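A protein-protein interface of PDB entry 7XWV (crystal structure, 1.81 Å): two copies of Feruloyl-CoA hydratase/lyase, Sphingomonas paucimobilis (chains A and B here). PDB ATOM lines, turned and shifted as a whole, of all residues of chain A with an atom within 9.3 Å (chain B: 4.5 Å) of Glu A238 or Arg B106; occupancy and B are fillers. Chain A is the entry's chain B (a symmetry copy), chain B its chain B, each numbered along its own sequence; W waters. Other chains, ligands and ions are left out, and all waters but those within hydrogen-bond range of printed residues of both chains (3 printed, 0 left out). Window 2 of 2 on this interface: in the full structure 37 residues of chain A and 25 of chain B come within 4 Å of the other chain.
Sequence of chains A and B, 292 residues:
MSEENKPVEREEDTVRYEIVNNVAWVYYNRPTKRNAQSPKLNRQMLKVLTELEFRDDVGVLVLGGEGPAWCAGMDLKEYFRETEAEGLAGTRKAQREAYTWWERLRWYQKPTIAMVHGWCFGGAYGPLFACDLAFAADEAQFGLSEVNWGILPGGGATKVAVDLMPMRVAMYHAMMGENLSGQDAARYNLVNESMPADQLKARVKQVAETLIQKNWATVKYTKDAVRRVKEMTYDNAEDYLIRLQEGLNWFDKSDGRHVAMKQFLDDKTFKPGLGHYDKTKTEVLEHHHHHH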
ATOM      1  N   VAL A 229      -1.581 -15.218 -26.865  1.00  0.00           N
ATOM      2  CA  VAL A 229      -2.943 -14.930 -27.383  1.00  0.00           C
ATOM      3  C   VAL A 229      -3.211 -13.422 -27.182  1.00  0.00           C
ATOM      4  O   VAL A 229      -4.145 -12.916 -27.768  1.00  0.00           O
ATOM      5  CB  VAL A 229      -4.009 -15.849 -26.797  1.00  0.00           C
ATOM      6  CG1 VAL A 229      -3.768 -17.284 -27.219  1.00  0.00           C
ATOM      7  CG2 VAL A 229      -4.120 -15.712 -25.293  1.00  0.00           C
ATOM      8  N   MET A 232      -3.062 -11.609 -30.635  1.00  0.00           N
ATOM      9  CA  MET A 232      -3.998 -12.313 -31.550  1.00  0.00           C
ATOM     10  C   MET A 232      -5.398 -11.767 -31.364  1.00  0.00           C
ATOM     11  O   MET A 232      -5.777 -11.390 -30.207  1.00  0.00           O
ATOM     12  CB  MET A 232      -4.078 -13.812 -31.254  1.00  0.00           C
ATOM     13  CG  MET A 232      -2.800 -14.489 -31.488  1.00  0.00           C
ATOM     14  SD  MET A 232      -2.979 -16.270 -31.318  1.00  0.00           S
ATOM     15  CE  MET A 232      -1.229 -16.619 -31.253  1.00  0.00           C
ATOM     16  N   THR A 233      -6.138 -11.745 -32.454  1.00  0.00           N
ATOM     17  CA  THR A 233      -7.596 -11.510 -32.392  1.00  0.00           C
ATOM     18  C   THR A 233      -8.256 -12.687 -31.655  1.00  0.00           C
ATOM     19  O   THR A 233      -7.691 -13.843 -31.632  1.00  0.00           O
ATOM     20  CB  THR A 233      -8.182 -11.290 -33.782  1.00  0.00           C
ATOM     21  OG1 THR A 233      -8.118 -12.539 -34.480  1.00  0.00           O
ATOM     22  CG2 THR A 233      -7.526 -10.141 -34.526  1.00  0.00           C
ATOM     23  N   TYR A 234      -9.421 -12.450 -31.077  1.00  0.00           N
ATOM     24  CA  TYR A 234     -10.150 -13.548 -30.406  1.00  0.00           C
ATOM     25  C   TYR A 234     -10.321 -14.740 -31.360  1.00  0.00           C
ATOM     26  O   TYR A 234     -10.121 -15.916 -30.986  1.00  0.00           O
ATOM     27  CB  TYR A 234     -11.464 -13.030 -29.859  1.00  0.00           C
ATOM     28  CG  TYR A 234     -12.198 -14.033 -29.004  1.00  0.00           C
ATOM     29  CD1 TYR A 234     -13.002 -15.010 -29.563  1.00  0.00           C
ATOM     30  CD2 TYR A 234     -12.118 -13.950 -27.624  1.00  0.00           C
ATOM     31  CE1 TYR A 234     -13.685 -15.922 -28.764  1.00  0.00           C
ATOM     32  CE2 TYR A 234     -12.831 -14.810 -26.820  1.00  0.00           C
ATOM     33  CZ  TYR A 234     -13.581 -15.824 -27.386  1.00  0.00           C
ATOM     34  OH  TYR A 234     -14.242 -16.685 -26.555  1.00  0.00           O
ATOM     35  N   ASP A 235     -10.773 -14.440 -32.564  1.00  0.00           N
ATOM     36  CA  ASP A 235     -11.074 -15.452 -33.590  1.00  0.00           C
ATOM     37  C   ASP A 235      -9.820 -16.278 -33.856  1.00  0.00           C
ATOM     38  O   ASP A 235      -9.967 -17.514 -33.908  1.00  0.00           O
ATOM     39  CB  ASP A 235     -11.546 -14.817 -34.893  1.00  0.00           C
ATOM     40  CG  ASP A 235     -12.172 -15.848 -35.802  1.00  0.00           C
ATOM     41  OD1 ASP A 235     -13.166 -16.450 -35.351  1.00  0.00           O
ATOM     42  OD2 ASP A 235     -11.619 -16.092 -36.922  1.00  0.00           O
ATOM     43  N   ASN A 236      -8.680 -15.619 -34.106  1.00  0.00           N
ATOM     44  CA  ASN A 236      -7.391 -16.320 -34.393  1.00  0.00           C
ATOM     45  C   ASN A 236      -6.919 -17.074 -33.147  1.00  0.00           C
ATOM     46  O   ASN A 236      -6.445 -18.198 -33.287  1.00  0.00           O
ATOM     47  CB  ASN A 236      -6.325 -15.398 -34.980  1.00  0.00           C
ATOM     48  CG  ASN A 236      -6.598 -15.126 -36.441  1.00  0.00           C
ATOM     49  OD1 ASN A 236      -7.310 -15.878 -37.099  1.00  0.00           O
ATOM     50  ND2 ASN A 236      -6.196 -13.968 -36.911  1.00  0.00           N
ATOM     51  N   ALA A 237      -7.138 -16.533 -31.963  1.00  0.00           N
ATOM     52  CA  ALA A 237      -6.775 -17.187 -30.694  1.00  0.00           C
ATOM     53  C   ALA A 237      -7.565 -18.487 -30.491  1.00  0.00           C
ATOM     54  O   ALA A 237      -6.980 -19.392 -29.933  1.00  0.00           O
ATOM     55  CB  ALA A 237      -6.982 -16.248 -29.551  1.00  0.00           C
ATOM     56  N   GLU A 238      -8.841 -18.588 -30.920  1.00  0.00           N
ATOM     57  CA  GLU A 238      -9.659 -19.809 -30.689  1.00  0.00           C
ATOM     58  C   GLU A 238      -9.011 -20.955 -31.461  1.00  0.00           C
ATOM     59  O   GLU A 238      -8.884 -22.058 -30.890  1.00  0.00           O
ATOM     60  CB  GLU A 238     -11.093 -19.718 -31.195  1.00  0.00           C
ATOM     61  CG  GLU A 238     -12.138 -19.547 -30.119  1.00  0.00           C
ATOM     62  CD  GLU A 238     -13.531 -19.337 -30.714  1.00  0.00           C
ATOM     63  OE1 GLU A 238     -13.673 -19.504 -31.933  1.00  0.00           O
ATOM     64  OE2 GLU A 238     -14.453 -19.009 -29.964  1.00  0.00           O
ATOM     65  N   ASP A 239      -8.646 -20.701 -32.730  1.00  0.00           N
ATOM     66  CA  ASP A 239      -8.050 -21.746 -33.596  1.00  0.00           C
ATOM     67  C   ASP A 239      -6.671 -22.134 -33.045  1.00  0.00           C
ATOM     68  O   ASP A 239      -6.375 -23.345 -32.928  1.00  0.00           O
ATOM     69  CB  ASP A 239      -8.027 -21.367 -35.067  1.00  0.00           C
ATOM     70  CG  ASP A 239      -7.581 -22.588 -35.851  1.00  0.00           C
ATOM     71  OD1 ASP A 239      -8.421 -23.498 -36.035  1.00  0.00           O
ATOM     72  OD2 ASP A 239      -6.387 -22.660 -36.160  1.00  0.00           O
ATOM     73  N   TYR A 240      -5.903 -21.137 -32.630  1.00  0.00           N
ATOM     74  CA  TYR A 240      -4.531 -21.286 -32.117  1.00  0.00           C
ATOM     75  C   TYR A 240      -4.530 -22.265 -30.937  1.00  0.00           C
ATOM     76  O   TYR A 240      -3.671 -23.155 -30.903  1.00  0.00           O
ATOM     77  CB  TYR A 240      -3.969 -19.930 -31.737  1.00  0.00           C
ATOM     78  CG  TYR A 240      -2.547 -19.965 -31.251  1.00  0.00           C
ATOM     79  CD1 TYR A 240      -1.493 -20.301 -32.085  1.00  0.00           C
ATOM     80  CD2 TYR A 240      -2.254 -19.695 -29.927  1.00  0.00           C
ATOM     81  CE1 TYR A 240      -0.178 -20.264 -31.653  1.00  0.00           C
ATOM     82  CE2 TYR A 240      -0.949 -19.642 -29.479  1.00  0.00           C
ATOM     83  CZ  TYR A 240       0.089 -19.953 -30.333  1.00  0.00           C
ATOM     84  OH  TYR A 240       1.351 -19.975 -29.857  1.00  0.00           O
ATOM     85  N   LEU A 241      -5.478 -22.115 -30.003  1.00  0.00           N
ATOM     86  CA  LEU A 241      -5.494 -22.939 -28.778  1.00  0.00           C
ATOM     87  C   LEU A 241      -5.806 -24.399 -29.127  1.00  0.00           C
ATOM     88  O   LEU A 241      -5.261 -25.261 -28.517  1.00  0.00           O
ATOM     89  CB  LEU A 241      -6.476 -22.328 -27.776  1.00  0.00           C
ATOM     90  CG  LEU A 241      -6.057 -20.972 -27.223  1.00  0.00           C
ATOM     91  CD1 LEU A 241      -7.246 -20.210 -26.648  1.00  0.00           C
ATOM     92  CD2 LEU A 241      -4.977 -21.131 -26.169  1.00  0.00           C
ATOM     93  N   ILE A 242      -6.592 -24.652 -30.167  1.00  0.00           N
ATOM     94  CA  ILE A 242      -6.840 -26.032 -30.666  1.00  0.00           C
ATOM     95  C   ILE A 242      -5.526 -26.584 -31.227  1.00  0.00           C
ATOM     96  O   ILE A 242      -5.194 -27.761 -30.903  1.00  0.00           O
ATOM     97  CB  ILE A 242      -7.960 -26.060 -31.716  1.00  0.00           C
ATOM     98  CG1 ILE A 242      -9.238 -25.423 -31.170  1.00  0.00           C
ATOM     99  CG2 ILE A 242      -8.157 -27.502 -32.200  1.00  0.00           C
ATOM    100  CD1 ILE A 242     -10.340 -25.169 -32.215  1.00  0.00           C
ATOM    101  N   ARG A 243      -4.838 -25.810 -32.074  1.00  0.00           N
ATOM    102  CA  ARG A 243      -3.510 -26.204 -32.643  1.00  0.00           C
ATOM    103  C   ARG A 243      -2.559 -26.502 -31.474  1.00  0.00           C
ATOM    104  O   ARG A 243      -1.905 -27.550 -31.487  1.00  0.00           O
ATOM    105  CB  ARG A 243      -2.940 -25.156 -33.589  1.00  0.00           C
ATOM    106  CG  ARG A 243      -3.802 -24.889 -34.813  1.00  0.00           C
ATOM    107  CD  ARG A 243      -3.868 -26.039 -35.807  1.00  0.00           C
ATOM    108  NE  ARG A 243      -4.888 -27.022 -35.483  1.00  0.00           N
ATOM    109  CZ  ARG A 243      -6.215 -26.839 -35.597  1.00  0.00           C
ATOM    110  NH1 ARG A 243      -7.038 -27.814 -35.247  1.00  0.00           N
ATOM    111  NH2 ARG A 243      -6.717 -25.672 -36.009  1.00  0.00           N
ATOM    112  N   LEU A 244      -2.603 -25.718 -30.406  1.00  0.00           N
ATOM    113  CA  LEU A 244      -1.655 -25.928 -29.297  1.00  0.00           C
ATOM    114  C   LEU A 244      -1.916 -27.288 -28.625  1.00  0.00           C
ATOM    115  O   LEU A 244      -0.931 -27.969 -28.321  1.00  0.00           O
ATOM    116  CB  LEU A 244      -1.746 -24.779 -28.294  1.00  0.00           C
ATOM    117  CG  LEU A 244      -1.097 -23.448 -28.701  1.00  0.00           C
ATOM    118  CD1 LEU A 244      -1.044 -22.528 -27.495  1.00  0.00           C
ATOM    119  CD2 LEU A 244       0.298 -23.618 -29.293  1.00  0.00           C
ATOM    120  N   GLN A 245      -3.177 -27.587 -28.278  1.00  0.00           N
ATOM    121  CA  GLN A 245      -3.588 -28.839 -27.595  1.00  0.00           C
ATOM    122  C   GLN A 245      -3.161 -30.050 -28.446  1.00  0.00           C
ATOM    123  O   GLN A 245      -2.735 -31.052 -27.863  1.00  0.00           O
ATOM    124  CB  GLN A 245      -5.094 -28.836 -27.288  1.00  0.00           C
ATOM    125  CG  GLN A 245      -5.561 -30.084 -26.570  1.00  0.00           C
ATOM    126  CD  GLN A 245      -4.919 -30.192 -25.218  1.00  0.00           C
ATOM    127  OE1 GLN A 245      -5.050 -29.304 -24.394  1.00  0.00           O
ATOM    128  NE2 GLN A 245      -4.182 -31.259 -24.993  1.00  0.00           N
ATOM    129  N   TYR B  99     -18.538 -23.951 -30.295  1.00  0.00           N
ATOM    130  CA  TYR B  99     -18.023 -22.651 -30.802  1.00  0.00           C
ATOM    131  C   TYR B  99     -19.165 -21.849 -31.435  1.00  0.00           C
ATOM    132  O   TYR B  99     -19.196 -20.648 -31.213  1.00  0.00           O
ATOM    133  CB  TYR B  99     -16.840 -22.807 -31.767  1.00  0.00           C
ATOM    134  CG  TYR B  99     -15.581 -23.218 -31.049  1.00  0.00           C
ATOM    135  CD1 TYR B  99     -15.001 -22.392 -30.099  1.00  0.00           C
ATOM    136  CD2 TYR B  99     -14.969 -24.427 -31.306  1.00  0.00           C
ATOM    137  CE1 TYR B  99     -13.848 -22.775 -29.421  1.00  0.00           C
ATOM    138  CE2 TYR B  99     -13.828 -24.830 -30.630  1.00  0.00           C
ATOM    139  CZ  TYR B  99     -13.276 -24.016 -29.667  1.00  0.00           C
ATOM    140  OH  TYR B  99     -12.141 -24.392 -29.014  1.00  0.00           O
ATOM    141  N   TRP B 102     -21.550 -20.130 -28.737  1.00  0.00           N
ATOM    142  CA  TRP B 102     -20.759 -19.053 -28.077  1.00  0.00           C
ATOM    143  C   TRP B 102     -20.714 -17.842 -29.000  1.00  0.00           C
ATOM    144  O   TRP B 102     -21.016 -16.781 -28.562  1.00  0.00           O
ATOM    145  CB  TRP B 102     -19.352 -19.532 -27.686  1.00  0.00           C
ATOM    146  CG  TRP B 102     -19.336 -20.731 -26.800  1.00  0.00           C
ATOM    147  CD1 TRP B 102     -20.373 -21.220 -26.063  1.00  0.00           C
ATOM    148  CD2 TRP B 102     -18.239 -21.626 -26.594  1.00  0.00           C
ATOM    149  NE1 TRP B 102     -19.973 -22.351 -25.400  1.00  0.00           N
ATOM    150  CE2 TRP B 102     -18.673 -22.624 -25.709  1.00  0.00           C
ATOM    151  CE3 TRP B 102     -16.911 -21.668 -27.058  1.00  0.00           C
ATOM    152  CZ2 TRP B 102     -17.847 -23.661 -25.279  1.00  0.00           C
ATOM    153  CZ3 TRP B 102     -16.108 -22.728 -26.684  1.00  0.00           C
ATOM    154  CH2 TRP B 102     -16.565 -23.686 -25.781  1.00  0.00           C
ATOM    155  N   GLU B 103     -20.401 -18.049 -30.274  1.00  0.00           N
ATOM    156  CA  GLU B 103     -20.306 -16.962 -31.278  1.00  0.00           C
ATOM    157  C   GLU B 103     -21.690 -16.294 -31.480  1.00  0.00           C
ATOM    158  O   GLU B 103     -21.713 -15.047 -31.576  1.00  0.00           O
ATOM    159  CB  GLU B 103     -19.734 -17.477 -32.606  1.00  0.00           C
ATOM    160  CG  GLU B 103     -19.607 -16.370 -33.649  1.00  0.00           C
ATOM    161  CD  GLU B 103     -18.960 -16.747 -34.981  1.00  0.00           C
ATOM    162  OE1 GLU B 103     -19.565 -17.577 -35.703  1.00  0.00           O
ATOM    163  OE2 GLU B 103     -17.850 -16.199 -35.305  1.00  0.00           O
ATOM    164  N   ARG B 104     -22.787 -17.061 -31.568  1.00  0.00           N
ATOM    165  CA  ARG B 104     -24.164 -16.531 -31.792  1.00  0.00           C
ATOM    166  C   ARG B 104     -24.437 -15.599 -30.611  1.00  0.00           C
ATOM    167  O   ARG B 104     -24.880 -14.450 -30.830  1.00  0.00           O
ATOM    168  CB  ARG B 104     -25.219 -17.640 -31.874  1.00  0.00           C
ATOM    169  CG  ARG B 104     -26.681 -17.166 -31.803  1.00  0.00           C
ATOM    170  CD  ARG B 104     -27.479 -17.319 -33.089  1.00  0.00           C
ATOM    171  NE  ARG B 104     -26.589 -17.271 -34.225  1.00  0.00           N
ATOM    172  CZ  ARG B 104     -26.486 -18.150 -35.214  1.00  0.00           C
ATOM    173  NH1 ARG B 104     -27.277 -19.205 -35.351  1.00  0.00           N
ATOM    174  NH2 ARG B 104     -25.554 -17.929 -36.110  1.00  0.00           N
ATOM    175  N   LEU B 105     -24.058 -16.037 -29.423  1.00  0.00           N
ATOM    176  CA  LEU B 105     -24.256 -15.237 -28.184  1.00  0.00           C
ATOM    177  C   LEU B 105     -23.362 -14.003 -28.219  1.00  0.00           C
ATOM    178  O   LEU B 105     -23.851 -12.892 -27.906  1.00  0.00           O
ATOM    179  CB  LEU B 105     -23.952 -16.112 -26.966  1.00  0.00           C
ATOM    180  CG  LEU B 105     -24.296 -15.457 -25.624  1.00  0.00           C
ATOM    181  CD1 LEU B 105     -25.764 -15.091 -25.541  1.00  0.00           C
ATOM    182  CD2 LEU B 105     -23.907 -16.361 -24.475  1.00  0.00           C
ATOM    183  N   ARG B 106     -22.093 -14.162 -28.637  1.00  0.00           N
ATOM    184  CA  ARG B 106     -21.102 -13.070 -28.545  1.00  0.00           C
ATOM    185  C   ARG B 106     -21.574 -11.898 -29.416  1.00  0.00           C
ATOM    186  O   ARG B 106     -21.369 -10.769 -29.014  1.00  0.00           O
ATOM    187  CB  ARG B 106     -19.736 -13.669 -28.880  1.00  0.00           C
ATOM    188  CG  ARG B 106     -18.581 -12.712 -28.704  1.00  0.00           C
ATOM    189  CD  ARG B 106     -17.265 -13.473 -28.613  1.00  0.00           C
ATOM    190  NE  ARG B 106     -17.019 -14.219 -29.841  1.00  0.00           N
ATOM    191  CZ  ARG B 106     -17.054 -15.545 -29.962  1.00  0.00           C
ATOM    192  NH1 ARG B 106     -17.226 -16.328 -28.925  1.00  0.00           N
ATOM    193  NH2 ARG B 106     -16.791 -16.097 -31.117  1.00  0.00           N
ATOM    194  N   TRP B 107     -22.196 -12.167 -30.575  1.00  0.00           N
ATOM    195  CA  TRP B 107     -22.643 -11.155 -31.566  1.00  0.00           C
ATOM    196  C   TRP B 107     -24.163 -11.004 -31.545  1.00  0.00           C
ATOM    197  O   TRP B 107     -24.750 -10.587 -32.563  1.00  0.00           O
ATOM    198  CB  TRP B 107     -22.102 -11.491 -32.960  1.00  0.00           C
ATOM    199  CG  TRP B 107     -20.612 -11.454 -32.906  1.00  0.00           C
ATOM    200  CD1 TRP B 107     -19.762 -12.512 -32.944  1.00  0.00           C
ATOM    201  CD2 TRP B 107     -19.810 -10.298 -32.625  1.00  0.00           C
ATOM    202  NE1 TRP B 107     -18.476 -12.084 -32.743  1.00  0.00           N
ATOM    203  CE2 TRP B 107     -18.477 -10.742 -32.513  1.00  0.00           C
ATOM    204  CE3 TRP B 107     -20.092  -8.945 -32.420  1.00  0.00           C
ATOM    205  CZ2 TRP B 107     -17.405  -9.867 -32.329  1.00  0.00           C
ATOM    206  CZ3 TRP B 107     -19.033  -8.079 -32.224  1.00  0.00           C
ATOM    207  CH2 TRP B 107     -17.717  -8.542 -32.154  1.00  0.00           C
ATOM    208  N   TYR B 108     -24.787 -11.236 -30.399  1.00  0.00           N
ATOM    209  CA  TYR B 108     -26.266 -11.321 -30.317  1.00  0.00           C
ATOM    210  C   TYR B 108     -26.875  -9.978 -30.737  1.00  0.00           C
ATOM    211  O   TYR B 108     -26.320  -8.893 -30.398  1.00  0.00           O
ATOM    212  CB  TYR B 108     -26.685 -11.734 -28.903  1.00  0.00           C
ATOM    213  CG  TYR B 108     -27.995 -12.478 -28.843  1.00  0.00           C
ATOM    214  CD1 TYR B 108     -28.147 -13.641 -29.580  1.00  0.00           C
ATOM    215  CD2 TYR B 108     -29.042 -12.065 -28.033  1.00  0.00           C
ATOM    216  CE1 TYR B 108     -29.306 -14.396 -29.509  1.00  0.00           C
ATOM    217  CE2 TYR B 108     -30.224 -12.785 -27.982  1.00  0.00           C
ATOM    218  CZ  TYR B 108     -30.341 -13.981 -28.685  1.00  0.00           C
ATOM    219  OH  TYR B 108     -31.479 -14.750 -28.683  1.00  0.00           O
ATOM    220  N   PHE B 129     -17.744 -14.728 -21.604  1.00  0.00           N
ATOM    221  CA  PHE B 129     -17.169 -13.621 -22.399  1.00  0.00           C
ATOM    222  C   PHE B 129     -18.195 -13.143 -23.455  1.00  0.00           C
ATOM    223  O   PHE B 129     -18.227 -11.930 -23.815  1.00  0.00           O
ATOM    224  CB  PHE B 129     -15.886 -14.109 -23.074  1.00  0.00           C
ATOM    225  CG  PHE B 129     -15.192 -13.067 -23.916  1.00  0.00           C
ATOM    226  CD1 PHE B 129     -14.301 -12.184 -23.336  1.00  0.00           C
ATOM    227  CD2 PHE B 129     -15.419 -12.963 -25.286  1.00  0.00           C
ATOM    228  CE1 PHE B 129     -13.635 -11.244 -24.099  1.00  0.00           C
ATOM    229  CE2 PHE B 129     -14.747 -12.009 -26.044  1.00  0.00           C
ATOM    230  CZ  PHE B 129     -13.861 -11.149 -25.445  1.00  0.00           C
ATOM    231  N   ALA B 130     -18.983 -14.092 -23.965  1.00  0.00           N
ATOM    232  CA  ALA B 130     -19.988 -13.902 -25.021  1.00  0.00           C
ATOM    233  C   ALA B 130     -21.142 -13.058 -24.471  1.00  0.00           C
ATOM    234  O   ALA B 130     -21.662 -12.227 -25.210  1.00  0.00           O
ATOM    235  CB  ALA B 130     -20.419 -15.249 -25.540  1.00  0.00           C
ATOM    236  N   ASP B 132     -22.365  -9.713 -22.745  1.00  0.00           N
ATOM    237  CA  ASP B 132     -21.824  -8.327 -22.780  1.00  0.00           C
ATOM    238  C   ASP B 132     -21.495  -7.891 -21.339  1.00  0.00           C
ATOM    239  O   ASP B 132     -20.420  -7.337 -21.119  1.00  0.00           O
ATOM    240  CB  ASP B 132     -22.799  -7.365 -23.431  1.00  0.00           C
ATOM    241  CG  ASP B 132     -23.179  -7.800 -24.828  1.00  0.00           C
ATOM    242  OD1 ASP B 132     -22.287  -8.321 -25.507  1.00  0.00           O
ATOM    243  OD2 ASP B 132     -24.386  -7.648 -25.217  1.00  0.00           O
ATOM    244  N   GLY B 156     -11.297 -21.098 -26.254  1.00  0.00           N
ATOM    245  CA  GLY B 156     -10.940 -19.682 -26.182  1.00  0.00           C
ATOM    246  C   GLY B 156     -10.768 -19.209 -24.744  1.00  0.00           C
ATOM    247  O   GLY B 156     -10.514 -18.016 -24.578  1.00  0.00           O
ATOM    248  N   ARG B 227     -16.813  -4.199 -28.503  1.00  0.00           N
ATOM    249  CA  ARG B 227     -16.102  -5.468 -28.770  1.00  0.00           C
ATOM    250  C   ARG B 227     -15.146  -5.281 -29.954  1.00  0.00           C
ATOM    251  O   ARG B 227     -14.023  -5.859 -29.925  1.00  0.00           O
ATOM    252  CB  ARG B 227     -17.080  -6.605 -29.078  1.00  0.00           C
ATOM    253  CG  ARG B 227     -17.962  -7.040 -27.931  1.00  0.00           C
ATOM    254  CD  ARG B 227     -18.746  -8.310 -28.312  1.00  0.00           C
ATOM    255  NE  ARG B 227     -19.529  -8.836 -27.213  1.00  0.00           N
ATOM    256  CZ  ARG B 227     -19.045  -9.575 -26.223  1.00  0.00           C
ATOM    257  NH1 ARG B 227     -17.761  -9.893 -26.181  1.00  0.00           N
ATOM    258  NH2 ARG B 227     -19.851  -9.984 -25.262  1.00  0.00           N
HETATM  259  O   HOH W   1      -9.990 -22.630 -28.694  1.00  0.00           O
HETATM  260  O   HOH W   2     -17.023 -19.098 -30.570  1.00  0.00           O
HETATM  261  O   HOH W   3     -16.845 -16.002 -26.299  1.00  0.00           O
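Water W1 lies within hydrogen-bond range of O of Glu A238, OH of Tyr B99 and N of Gly B156. Water W2 lies within hydrogen-bond range of the side-chain carboxylate (OE2) of Glu A238 (2.6 Å), the backbone carbonyl oxygen (O) of Tyr B99 (2.7 Å) and the guanidinium group (NH2) of Arg B106 (3.1 Å). Water W3 bridges the guanidinium group (NH1) of Arg B106 (2.7 Å) and the side-chain hydroxyl (OH) of Tyr A234 (2.7 Å).
Of chain B, only Tyr B99 and Arg B106 come within 4 Å of Glu A238. Printed residues of chain A within 4 Å of Arg B106: Tyr A234 and Glu A238. No residue of chain A comes within 4 Å of Leu B105. Ala B130 touches none of the printed residues of chain A. Printed residues of chain B within 4 Å of Tyr A234: Arg B106 (3.6 Å) and Phe B129 (3.5 Å). Printed residues of chain B within 4 Å of Leu A241: Gly B156. Of the printed residues of chain B, Ile A242 touches Tyr B99 (3.8 Å). Printed residues of chain A within 4 Å of Tyr B99: Glu A238 and Ile A242. Of the printed residues of chain A, Gly B156 touches Leu A241. Asp A239 touches none of the printed residues of chain B. Tyr B108 touches none of the printed residues of chain A.
The guanidinium group of Arg B106 lies within salt-bridge range of the side-chain carboxylate of Glu A238 (3.9 Å).
Among the printed residues, pairs that only touch across the chains: Glu A238 with Tyr B99, Tyr A234 with Phe B129, Tyr A234 with Arg B106, Ile A242 with Tyr B99 and Leu A241 with Gly B156.
No position is printed for both chains. Of the 6 pairs that touch across the chains among the printed residues, none has its exchanged pair printed and touching as well.
The backbone carbonyl oxygen (O) of Phe B129 is in hydrogen-bond range of the guanidinium group (NH2) of Arg B227. The backbone carbonyl oxygen (O) of Arg B106 is in hydrogen-bond range of the guanidinium group (NE) of Arg B227, 3.2 Å away.
Hydrophobic or aromatic side chains of chain A that line the printed part of chain B: Tyr A234, Leu A241 and Ile A242. Hydrophobic or aromatic side chains of chain B within 4 Å of the printed part of chain A: Tyr B99 and Phe B129. Among the printed residues, Asp or Glu carboxylates within 4 Å of a Lys or Arg side-chain nitrogen of the other chain: Glu A238 with Arg B106.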
